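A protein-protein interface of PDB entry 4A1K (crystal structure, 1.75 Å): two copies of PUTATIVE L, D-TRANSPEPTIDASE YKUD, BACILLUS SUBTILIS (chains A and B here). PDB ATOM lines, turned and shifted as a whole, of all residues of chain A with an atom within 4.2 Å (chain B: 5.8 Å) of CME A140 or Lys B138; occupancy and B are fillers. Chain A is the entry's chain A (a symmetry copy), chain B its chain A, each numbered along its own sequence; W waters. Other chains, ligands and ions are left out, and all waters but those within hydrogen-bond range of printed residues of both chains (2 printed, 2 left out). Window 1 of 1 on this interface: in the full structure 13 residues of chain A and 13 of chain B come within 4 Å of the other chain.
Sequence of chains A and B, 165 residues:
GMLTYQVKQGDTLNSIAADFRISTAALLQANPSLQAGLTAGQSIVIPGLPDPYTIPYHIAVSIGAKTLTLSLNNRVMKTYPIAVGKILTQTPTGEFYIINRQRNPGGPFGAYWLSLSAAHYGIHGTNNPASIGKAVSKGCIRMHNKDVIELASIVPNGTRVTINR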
ATOM      1  N   ALA A  83      -9.778 -25.068 -18.774  1.00  0.00           N
ATOM      2  CA  ALA A  83     -11.144 -24.696 -18.432  1.00  0.00           C
ATOM      3  C   ALA A  83     -11.907 -24.422 -19.732  1.00  0.00           C
ATOM      4  O   ALA A  83     -11.324 -23.946 -20.705  1.00  0.00           O
ATOM      5  CB  ALA A  83     -11.162 -23.464 -17.519  1.00  0.00           C
ATOM      6  N   THR A  91     -17.961 -23.178 -24.928  1.00  0.00           N
ATOM      7  CA  THR A  91     -16.882 -23.097 -25.897  1.00  0.00           C
ATOM      8  C   THR A  91     -17.416 -23.608 -27.237  1.00  0.00           C
ATOM      9  O   THR A  91     -18.029 -24.675 -27.301  1.00  0.00           O
ATOM     10  CB  THR A  91     -15.686 -23.954 -25.429  1.00  0.00           C
ATOM     11  OG1 THR A  91     -15.170 -23.425 -24.199  1.00  0.00           O
ATOM     12  CG2 THR A  91     -14.587 -23.977 -26.488  1.00  0.00           C
ATOM     13  N   PHE A 109      -6.811 -12.952 -18.245  1.00  0.00           N
ATOM     14  CA  PHE A 109      -6.136 -13.541 -19.399  1.00  0.00           C
ATOM     15  C   PHE A 109      -4.746 -14.054 -19.046  1.00  0.00           C
ATOM     16  O   PHE A 109      -4.142 -14.792 -19.809  1.00  0.00           O
ATOM     17  CB  PHE A 109      -6.045 -12.513 -20.531  1.00  0.00           C
ATOM     18  CG  PHE A 109      -7.322 -11.761 -20.749  1.00  0.00           C
ATOM     19  CD1 PHE A 109      -8.451 -12.416 -21.236  1.00  0.00           C
ATOM     20  CD2 PHE A 109      -7.413 -10.414 -20.430  1.00  0.00           C
ATOM     21  CE1 PHE A 109      -9.642 -11.728 -21.426  1.00  0.00           C
ATOM     22  CE2 PHE A 109      -8.601  -9.722 -20.607  1.00  0.00           C
ATOM     23  CZ  PHE A 109      -9.719 -10.384 -21.104  1.00  0.00           C
ATOM     24  N   TRP A 113      -2.439 -14.353 -24.447  1.00  0.00           N
ATOM     25  CA  TRP A 113      -3.711 -14.490 -25.154  1.00  0.00           C
ATOM     26  C   TRP A 113      -3.409 -14.935 -26.598  1.00  0.00           C
ATOM     27  O   TRP A 113      -2.568 -14.326 -27.262  1.00  0.00           O
ATOM     28  CB  TRP A 113      -4.469 -13.151 -25.177  1.00  0.00           C
ATOM     29  CG  TRP A 113      -5.597 -13.121 -26.192  1.00  0.00           C
ATOM     30  CD1 TRP A 113      -5.486 -12.893 -27.539  1.00  0.00           C
ATOM     31  CD2 TRP A 113      -6.990 -13.356 -25.940  1.00  0.00           C
ATOM     32  NE1 TRP A 113      -6.728 -12.982 -28.140  1.00  0.00           N
ATOM     33  CE2 TRP A 113      -7.667 -13.246 -27.180  1.00  0.00           C
ATOM     34  CE3 TRP A 113      -7.735 -13.616 -24.786  1.00  0.00           C
ATOM     35  CZ2 TRP A 113      -9.046 -13.416 -27.298  1.00  0.00           C
ATOM     36  CZ3 TRP A 113      -9.114 -13.779 -24.908  1.00  0.00           C
ATOM     37  CH2 TRP A 113      -9.750 -13.679 -26.160  1.00  0.00           C
ATOM     38  N   HIS A 120     -14.199 -12.711 -30.603  1.00  0.00           N
ATOM     39  CA  HIS A 120     -14.160 -12.619 -29.139  1.00  0.00           C
ATOM     40  C   HIS A 120     -13.640 -13.853 -28.408  1.00  0.00           C
ATOM     41  O   HIS A 120     -13.595 -13.851 -27.173  1.00  0.00           O
ATOM     42  CB  HIS A 120     -15.536 -12.257 -28.558  1.00  0.00           C
ATOM     43  CG  HIS A 120     -16.250 -11.193 -29.328  1.00  0.00           C
ATOM     44  ND1 HIS A 120     -15.814  -9.885 -29.362  1.00  0.00           N
ATOM     45  CD2 HIS A 120     -17.354 -11.246 -30.112  1.00  0.00           C
ATOM     46  CE1 HIS A 120     -16.619  -9.177 -30.136  1.00  0.00           C
ATOM     47  NE2 HIS A 120     -17.565  -9.976 -30.598  1.00  0.00           N
ATOM     48  N   TYR A 121     -13.251 -14.897 -29.130  1.00  0.00           N
ATOM     49  CA  TYR A 121     -12.763 -16.112 -28.474  1.00  0.00           C
ATOM     50  C   TYR A 121     -11.256 -16.296 -28.626  1.00  0.00           C
ATOM     51  O   TYR A 121     -10.649 -15.847 -29.605  1.00  0.00           O
ATOM     52  CB  TYR A 121     -13.486 -17.354 -29.000  1.00  0.00           C
ATOM     53  CG  TYR A 121     -14.937 -17.395 -28.592  1.00  0.00           C
ATOM     54  CD1 TYR A 121     -15.326 -17.908 -27.360  1.00  0.00           C
ATOM     55  CD2 TYR A 121     -15.920 -16.909 -29.431  1.00  0.00           C
ATOM     56  CE1 TYR A 121     -16.667 -17.939 -26.986  1.00  0.00           C
ATOM     57  CE2 TYR A 121     -17.265 -16.942 -29.072  1.00  0.00           C
ATOM     58  CZ  TYR A 121     -17.632 -17.451 -27.849  1.00  0.00           C
ATOM     59  OH  TYR A 121     -18.965 -17.469 -27.487  1.00  0.00           O
ATOM     60  N   GLY A 122     -10.660 -16.955 -27.644  1.00  0.00           N
ATOM     61  CA  GLY A 122      -9.238 -17.216 -27.675  1.00  0.00           C
ATOM     62  C   GLY A 122      -8.830 -18.292 -26.690  1.00  0.00           C
ATOM     63  O   GLY A 122      -9.656 -18.822 -25.939  1.00  0.00           O
ATOM     64  N   HIS A 124      -6.274 -18.629 -23.525  1.00  0.00           N
ATOM     65  CA  HIS A 124      -5.488 -17.748 -22.661  1.00  0.00           C
ATOM     66  C   HIS A 124      -5.070 -18.397 -21.348  1.00  0.00           C
ATOM     67  O   HIS A 124      -5.423 -19.545 -21.073  1.00  0.00           O
ATOM     68  CB  HIS A 124      -6.157 -16.364 -22.471  1.00  0.00           C
ATOM     69  CG  HIS A 124      -7.505 -16.375 -21.801  1.00  0.00           C
ATOM     70  ND1 HIS A 124      -7.680 -16.629 -20.453  1.00  0.00           N
ATOM     71  CD2 HIS A 124      -8.732 -16.064 -22.283  1.00  0.00           C
ATOM     72  CE1 HIS A 124      -8.961 -16.512 -20.148  1.00  0.00           C
ATOM     73  NE2 HIS A 124      -9.619 -16.159 -21.239  1.00  0.00           N
ATOM     74  N   SER A 137     -15.903 -21.183 -17.754  1.00  0.00           N
ATOM     75  CA  SER A 137     -15.497 -19.999 -18.519  1.00  0.00           C
ATOM     76  C   SER A 137     -16.637 -19.356 -19.326  1.00  0.00           C
ATOM     77  O   SER A 137     -17.740 -19.896 -19.413  1.00  0.00           O
ATOM     78  CB  SER A 137     -14.336 -20.349 -19.452  1.00  0.00           C
ATOM     79  OG  SER A 137     -14.804 -20.798 -20.714  1.00  0.00           O
ATOM     80  N   LYS A 138     -16.353 -18.195 -19.921  1.00  0.00           N
ATOM     81  CA  LYS A 138     -17.308 -17.508 -20.785  1.00  0.00           C
ATOM     82  C   LYS A 138     -17.301 -18.128 -22.188  1.00  0.00           C
ATOM     83  O   LYS A 138     -18.064 -17.718 -23.075  1.00  0.00           O
ATOM     84  CB  LYS A 138     -16.972 -16.007 -20.862  1.00  0.00           C
ATOM     85  CG  LYS A 138     -18.054 -15.155 -21.542  1.00  0.00           C
ATOM     86  CD  LYS A 138     -17.619 -13.687 -21.640  1.00  0.00           C
ATOM     87  CE  LYS A 138     -18.618 -12.834 -22.435  1.00  0.00           C
ATOM     88  NZ  LYS A 138     -18.250 -11.366 -22.377  1.00  0.00           N
ATOM     89  N   GLY A 139     -16.435 -19.117 -22.390  1.00  0.00           N
ATOM     90  CA  GLY A 139     -16.303 -19.757 -23.695  1.00  0.00           C
ATOM     91  C   GLY A 139     -14.861 -19.903 -24.157  1.00  0.00           C
ATOM     92  O   GLY A 139     -14.546 -20.801 -24.955  1.00  0.00           O
ATOM     93  N   CME A 140     -13.984 -19.013 -23.685  1.00  0.00           N
ATOM     94  CA  CME A 140     -12.622 -19.085 -24.019  1.00  0.00           C
ATOM     95  CB  CME A 140     -11.881 -17.906 -23.485  1.00  0.00           C
ATOM     96  SG  CME A 140     -12.193 -16.384 -24.382  1.00  0.00           S
ATOM     97  SD  CME A 140     -13.904 -15.721 -23.562  1.00  0.00           S
ATOM     98  CE  CME A 140     -15.246 -15.938 -24.718  1.00  0.00           C
ATOM     99  CZ  CME A 140     -15.799 -14.716 -25.373  1.00  0.00           C
ATOM    100  OH  CME A 140     -15.753 -13.547 -24.676  1.00  0.00           O
ATOM    101  C   CME A 140     -12.042 -20.286 -23.394  1.00  0.00           C
ATOM    102  O   CME A 140     -12.584 -20.832 -22.421  1.00  0.00           O
ATOM    103  N   ILE A 141     -10.919 -20.732 -23.940  1.00  0.00           N
ATOM    104  CA  ILE A 141     -10.186 -21.862 -23.376  1.00  0.00           C
ATOM    105  C   ILE A 141      -9.124 -21.315 -22.427  1.00  0.00           C
ATOM    106  O   ILE A 141      -8.257 -20.548 -22.845  1.00  0.00           O
ATOM    107  CB  ILE A 141      -9.511 -22.695 -24.495  1.00  0.00           C
ATOM    108  CG1 ILE A 141     -10.570 -23.406 -25.354  1.00  0.00           C
ATOM    109  CG2 ILE A 141      -8.520 -23.698 -23.902  1.00  0.00           C
ATOM    110  CD1 ILE A 141     -10.060 -23.881 -26.700  1.00  0.00           C
ATOM    111  N   ARG A 142      -9.197 -21.691 -21.150  1.00  0.00           N
ATOM    112  CA  ARG A 142      -8.196 -21.247 -20.170  1.00  0.00           C
ATOM    113  C   ARG A 142      -7.173 -22.334 -19.896  1.00  0.00           C
ATOM    114  O   ARG A 142      -7.513 -23.514 -19.848  1.00  0.00           O
ATOM    115  CB  ARG A 142      -8.812 -20.851 -18.826  1.00  0.00           C
ATOM    116  CG  ARG A 142      -9.973 -19.899 -18.896  1.00  0.00           C
ATOM    117  CD  ARG A 142     -10.420 -19.598 -17.473  1.00  0.00           C
ATOM    118  NE  ARG A 142     -11.551 -18.685 -17.456  1.00  0.00           N
ATOM    119  CZ  ARG A 142     -12.193 -18.302 -16.360  1.00  0.00           C
ATOM    120  NH1 ARG A 142     -11.816 -18.754 -15.173  1.00  0.00           N
ATOM    121  NH2 ARG A 142     -13.214 -17.458 -16.461  1.00  0.00           N
ATOM    122  N   VAL B  84     -21.901  -6.149 -14.341  1.00  0.00           N
ATOM    123  CA  VAL B  84     -20.490  -5.748 -14.306  1.00  0.00           C
ATOM    124  C   VAL B  84     -19.652  -6.932 -13.827  1.00  0.00           C
ATOM    125  O   VAL B  84     -20.194  -7.972 -13.482  1.00  0.00           O
ATOM    126  CB  VAL B  84     -20.248  -4.524 -13.396  1.00  0.00           C
ATOM    127  CG1 VAL B  84     -20.993  -3.303 -13.930  1.00  0.00           C
ATOM    128  CG2 VAL B  84     -20.660  -4.832 -11.957  1.00  0.00           C
ATOM    129  N   GLY B  85     -18.333  -6.782 -13.829  1.00  0.00           N
ATOM    130  CA  GLY B  85     -17.458  -7.904 -13.534  1.00  0.00           C
ATOM    131  C   GLY B  85     -17.490  -8.390 -12.095  1.00  0.00           C
ATOM    132  O   GLY B  85     -17.615  -7.603 -11.154  1.00  0.00           O
ATOM    133  N   LYS B  86     -17.357  -9.699 -11.923  1.00  0.00           N
ATOM    134  CA  LYS B  86     -17.204 -10.272 -10.588  1.00  0.00           C
ATOM    135  C   LYS B  86     -15.817  -9.960 -10.020  1.00  0.00           C
ATOM    136  O   LYS B  86     -14.975  -9.377 -10.704  1.00  0.00           O
ATOM    137  CB  LYS B  86     -17.472 -11.777 -10.617  1.00  0.00           C
ATOM    138  CG  LYS B  86     -16.584 -12.548 -11.564  1.00  0.00           C
ATOM    139  CD  LYS B  86     -17.113 -13.956 -11.796  1.00  0.00           C
ATOM    140  CE  LYS B  86     -16.158 -14.763 -12.669  1.00  0.00           C
ATOM    141  NZ  LYS B  86     -15.965 -14.194 -14.045  1.00  0.00           N
ATOM    142  N   THR B  89     -12.616 -10.854 -11.833  1.00  0.00           N
ATOM    143  CA  THR B  89     -12.618 -10.399 -13.221  1.00  0.00           C
ATOM    144  C   THR B  89     -13.391  -9.080 -13.342  1.00  0.00           C
ATOM    145  O   THR B  89     -14.405  -8.988 -14.032  1.00  0.00           O
ATOM    146  CB  THR B  89     -13.214 -11.459 -14.176  1.00  0.00           C
ATOM    147  OG1 THR B  89     -14.594 -11.677 -13.863  1.00  0.00           O
ATOM    148  CG2 THR B  89     -12.463 -12.783 -14.051  1.00  0.00           C
ATOM    149  N   GLN B  90     -12.909  -8.054 -12.656  1.00  0.00           N
ATOM    150  CA  GLN B  90     -13.682  -6.825 -12.560  1.00  0.00           C
ATOM    151  C   GLN B  90     -13.717  -6.011 -13.845  1.00  0.00           C
ATOM    152  O   GLN B  90     -12.831  -6.111 -14.696  1.00  0.00           O
ATOM    153  CB  GLN B  90     -13.183  -5.976 -11.389  1.00  0.00           C
ATOM    154  CG  GLN B  90     -13.393  -6.674 -10.066  1.00  0.00           C
ATOM    155  CD  GLN B  90     -12.854  -5.877  -8.907  1.00  0.00           C
ATOM    156  OE1 GLN B  90     -12.855  -4.647  -8.933  1.00  0.00           O
ATOM    157  NE2 GLN B  90     -12.382  -6.576  -7.880  1.00  0.00           N
ATOM    158  N   THR B  91     -14.760  -5.202 -13.971  1.00  0.00           N
ATOM    159  CA  THR B  91     -14.834  -4.220 -15.040  1.00  0.00           C
ATOM    160  C   THR B  91     -13.772  -3.151 -14.769  1.00  0.00           C
ATOM    161  O   THR B  91     -13.677  -2.632 -13.655  1.00  0.00           O
ATOM    162  CB  THR B  91     -16.241  -3.586 -15.080  1.00  0.00           C
ATOM    163  OG1 THR B  91     -17.212  -4.597 -15.387  1.00  0.00           O
ATOM    164  CG2 THR B  91     -16.305  -2.470 -16.118  1.00  0.00           C
ATOM    165  N   PRO B 108     -23.325 -15.241 -25.748  1.00  0.00           N
ATOM    166  CA  PRO B 108     -23.450 -14.406 -24.552  1.00  0.00           C
ATOM    167  C   PRO B 108     -23.512 -12.919 -24.889  1.00  0.00           C
ATOM    168  O   PRO B 108     -23.816 -12.102 -24.017  1.00  0.00           O
ATOM    169  CB  PRO B 108     -22.172 -14.720 -23.758  1.00  0.00           C
ATOM    170  CG  PRO B 108     -21.204 -15.264 -24.755  1.00  0.00           C
ATOM    171  CD  PRO B 108     -22.040 -15.963 -25.809  1.00  0.00           C
ATOM    172  N   PHE B 109     -23.205 -12.569 -26.136  1.00  0.00           N
ATOM    173  CA  PHE B 109     -23.111 -11.168 -26.539  1.00  0.00           C
ATOM    174  C   PHE B 109     -24.458 -10.609 -26.979  1.00  0.00           C
ATOM    175  O   PHE B 109     -24.622  -9.406 -27.107  1.00  0.00           O
ATOM    176  CB  PHE B 109     -22.087 -11.016 -27.668  1.00  0.00           C
ATOM    177  CG  PHE B 109     -20.823 -11.782 -27.424  1.00  0.00           C
ATOM    178  CD1 PHE B 109     -19.962 -11.410 -26.393  1.00  0.00           C
ATOM    179  CD2 PHE B 109     -20.511 -12.896 -28.189  1.00  0.00           C
ATOM    180  CE1 PHE B 109     -18.796 -12.125 -26.151  1.00  0.00           C
ATOM    181  CE2 PHE B 109     -19.355 -13.621 -27.948  1.00  0.00           C
ATOM    182  CZ  PHE B 109     -18.497 -13.235 -26.923  1.00  0.00           C
ATOM    183  N   TYR B 121     -12.406  -6.017 -24.082  1.00  0.00           N
ATOM    184  CA  TYR B 121     -13.578  -5.525 -23.354  1.00  0.00           C
ATOM    185  C   TYR B 121     -14.564  -4.790 -24.257  1.00  0.00           C
ATOM    186  O   TYR B 121     -14.186  -4.198 -25.274  1.00  0.00           O
ATOM    187  CB  TYR B 121     -13.166  -4.613 -22.196  1.00  0.00           C
ATOM    188  CG  TYR B 121     -12.461  -5.359 -21.093  1.00  0.00           C
ATOM    189  CD1 TYR B 121     -13.174  -6.011 -20.092  1.00  0.00           C
ATOM    190  CD2 TYR B 121     -11.082  -5.427 -21.055  1.00  0.00           C
ATOM    191  CE1 TYR B 121     -12.518  -6.704 -19.078  1.00  0.00           C
ATOM    192  CE2 TYR B 121     -10.415  -6.110 -20.041  1.00  0.00           C
ATOM    193  CZ  TYR B 121     -11.135  -6.751 -19.061  1.00  0.00           C
ATOM    194  OH  TYR B 121     -10.473  -7.441 -18.065  1.00  0.00           O
ATOM    195  N   VAL B 136     -21.587 -10.218 -12.091  1.00  0.00           N
ATOM    196  CA  VAL B 136     -21.365 -11.611 -12.463  1.00  0.00           C
ATOM    197  C   VAL B 136     -20.634 -11.806 -13.795  1.00  0.00           C
ATOM    198  O   VAL B 136     -20.482 -12.936 -14.261  1.00  0.00           O
ATOM    199  CB  VAL B 136     -22.702 -12.395 -12.507  1.00  0.00           C
ATOM    200  CG1 VAL B 136     -23.345 -12.388 -11.138  1.00  0.00           C
ATOM    201  CG2 VAL B 136     -23.644 -11.796 -13.547  1.00  0.00           C
ATOM    202  N   SER B 137     -20.151 -10.719 -14.392  1.00  0.00           N
ATOM    203  CA  SER B 137     -19.526 -10.813 -15.717  1.00  0.00           C
ATOM    204  C   SER B 137     -18.008 -11.058 -15.675  1.00  0.00           C
ATOM    205  O   SER B 137     -17.387 -11.027 -14.612  1.00  0.00           O
ATOM    206  CB  SER B 137     -19.825  -9.552 -16.530  1.00  0.00           C
ATOM    207  OG  SER B 137     -18.838  -8.555 -16.319  1.00  0.00           O
ATOM    208  N   LYS B 138     -17.420 -11.296 -16.848  1.00  0.00           N
ATOM    209  CA  LYS B 138     -15.975 -11.466 -16.975  1.00  0.00           C
ATOM    210  C   LYS B 138     -15.276 -10.100 -17.002  1.00  0.00           C
ATOM    211  O   LYS B 138     -14.042 -10.012 -17.071  1.00  0.00           O
ATOM    212  CB  LYS B 138     -15.643 -12.261 -18.253  1.00  0.00           C
ATOM    213  CG  LYS B 138     -14.177 -12.706 -18.351  1.00  0.00           C
ATOM    214  CD  LYS B 138     -13.909 -13.432 -19.677  1.00  0.00           C
ATOM    215  CE  LYS B 138     -12.424 -13.772 -19.867  1.00  0.00           C
ATOM    216  NZ  LYS B 138     -12.213 -14.627 -21.098  1.00  0.00           N
ATOM    217  N   GLY B 139     -16.069  -9.033 -16.949  1.00  0.00           N
ATOM    218  CA  GLY B 139     -15.527  -7.680 -17.012  1.00  0.00           C
ATOM    219  C   GLY B 139     -16.254  -6.778 -17.999  1.00  0.00           C
ATOM    220  O   GLY B 139     -16.253  -5.547 -17.841  1.00  0.00           O
ATOM    221  N   CME B 140     -16.854  -7.376 -19.031  1.00  0.00           N
ATOM    222  CA  CME B 140     -17.584  -6.637 -19.976  1.00  0.00           C
ATOM    223  CB  CME B 140     -18.035  -7.509 -21.099  1.00  0.00           C
ATOM    224  SG  CME B 140     -16.722  -7.973 -22.230  1.00  0.00           S
ATOM    225  SD  CME B 140     -15.869  -9.544 -21.310  1.00  0.00           S
ATOM    226  CE  CME B 140     -14.280  -9.064 -20.656  1.00  0.00           C
ATOM    227  CZ  CME B 140     -13.062  -9.585 -21.346  1.00  0.00           C
ATOM    228  OH  CME B 140     -13.151 -10.798 -21.958  1.00  0.00           O
ATOM    229  C   CME B 140     -18.794  -6.100 -19.327  1.00  0.00           C
ATOM    230  O   CME B 140     -19.245  -6.604 -18.287  1.00  0.00           O
ATOM    231  N   ARG B 142     -22.662  -5.778 -19.495  1.00  0.00           N
ATOM    232  CA  ARG B 142     -23.829  -6.397 -20.140  1.00  0.00           C
ATOM    233  C   ARG B 142     -25.070  -5.541 -19.971  1.00  0.00           C
ATOM    234  O   ARG B 142     -25.272  -4.933 -18.922  1.00  0.00           O
ATOM    235  CB  ARG B 142     -24.151  -7.785 -19.582  1.00  0.00           C
ATOM    236  CG  ARG B 142     -22.995  -8.742 -19.503  1.00  0.00           C
ATOM    237  CD  ARG B 142     -23.516 -10.065 -18.965  1.00  0.00           C
ATOM    238  NE  ARG B 142     -22.449 -11.047 -18.851  1.00  0.00           N
ATOM    239  CZ  ARG B 142     -22.598 -12.265 -18.347  1.00  0.00           C
ATOM    240  NH1 ARG B 142     -23.780 -12.664 -17.901  1.00  0.00           N
ATOM    241  NH2 ARG B 142     -21.552 -13.083 -18.295  1.00  0.00           N
HETATM  242  O   HOH W   1     -14.754 -16.707 -14.296  1.00  0.00           O
HETATM  243  O   HOH W   2     -15.784 -15.561 -16.988  1.00  0.00           O
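Of chain B, only Phe B109 and Lys B138 come within 4 Å of CME A140. Of chain A, only Phe A109, His A124 and CME A140 come within 4 Å of Lys B138. Of the printed residues of chain A, Pro B108 touches Tyr A121. Of the printed residues of chain B, His A124 touches Lys B138. Of the printed residues of chain B, Tyr A121 touches Pro B108 (3.8 Å) and Phe B109 (3.9 Å). Gln B90 touches none of the printed residues of chain A. The nearest printed residue of chain A that does not touch Lys B138 is Lys A138 (4.2 Å).
Phe A109 touches Tyr B121, and with the chains exchanged Tyr A121 touches Phe B109. Phe A109 touches Lys B138, and with the chains exchanged Lys A138 touches Phe B109. Phe A109 touches CME B140, and with the chains exchanged CME A140 touches Phe B109. Lys A138 touches CME B140, and with the chains exchanged CME A140 touches Lys B138. 8 positions are printed for both chains. Of the 11 pairs that touch across the chains among the printed residues, 8 have their exchanged pair printed and touching as well.
Hydrophobic or aromatic side chains of chain A within 4 Å of the printed part of chain B: Phe A109, His A120, Tyr A121 and His A124. Along chain A the printed residues that touch a printed residue of chain B span positions 109 to 140. Printed residues of chain B that touch a printed residue of chain A: Pro B108, Phe B109, Tyr B121, Lys B138 and CME B140. Hydrophobic or aromatic side chains of chain B within 4 Å of the printed part of chain A: Pro B108, Phe B109 and Tyr B121. Among the printed residues, 11 pairs touch across the chains. Among the printed residues, no Asp or Glu carboxylate lies within 4 Å of a Lys or Arg side-chain nitrogen of the other chain.
CE2 of Phe A109 touches OH of Tyr B121 (3.9 Å). Lys B138 touches Phe A109. Phe A109 touches CME B140 (CZ to CZ, 3.4 Å). Phe B109 touches His A120 (CZ to CB, 3.5 Å). Tyr A121 touches Pro B108. Tyr A121 touches Phe B109 (OH to CE2, 3.9 Å). Lys A138 touches Phe B109. CZ of Phe B109 touches CZ of CME A140, 3.4 Å away.
O of CME B140 lies within hydrogen-bond range of OG of Ser B137, 2.8 Å away. OH of CME A140 lies close to the backbone carbonyl oxygen (O) of His A120 (3.3 Å). N of Gly A122 is in hydrogen-bond range of SG of CME A140. The backbone carbonyl oxygen (O) of Ile A141 lies within hydrogen-bond range of the backbone NH (N) of His A124 (2.8 Å). OG of Ser A137 sits at hydrogen-bond distance from O of CME A140.
Water W1 bridges NH2 of Arg A142 (2.8 Å) and NZ of Lys B86 (2.8 Å). Water W2 lies within hydrogen-bond range of the guanidinium group of Arg A142 and the side-chain amino group of Lys B86.
The side-chain amino group (NZ) of Lys B138 sits at hydrogen-bond distance from a ring nitrogen (NE2) of His A124. The side-chain amino group (NZ) of Lys B138 lies within hydrogen-bond range of SD of CME A140, 3.2 Å away. The side-chain amino group (NZ) of Lys A138 lies within hydrogen-bond range of SD of CME B140 (3.2 Å).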
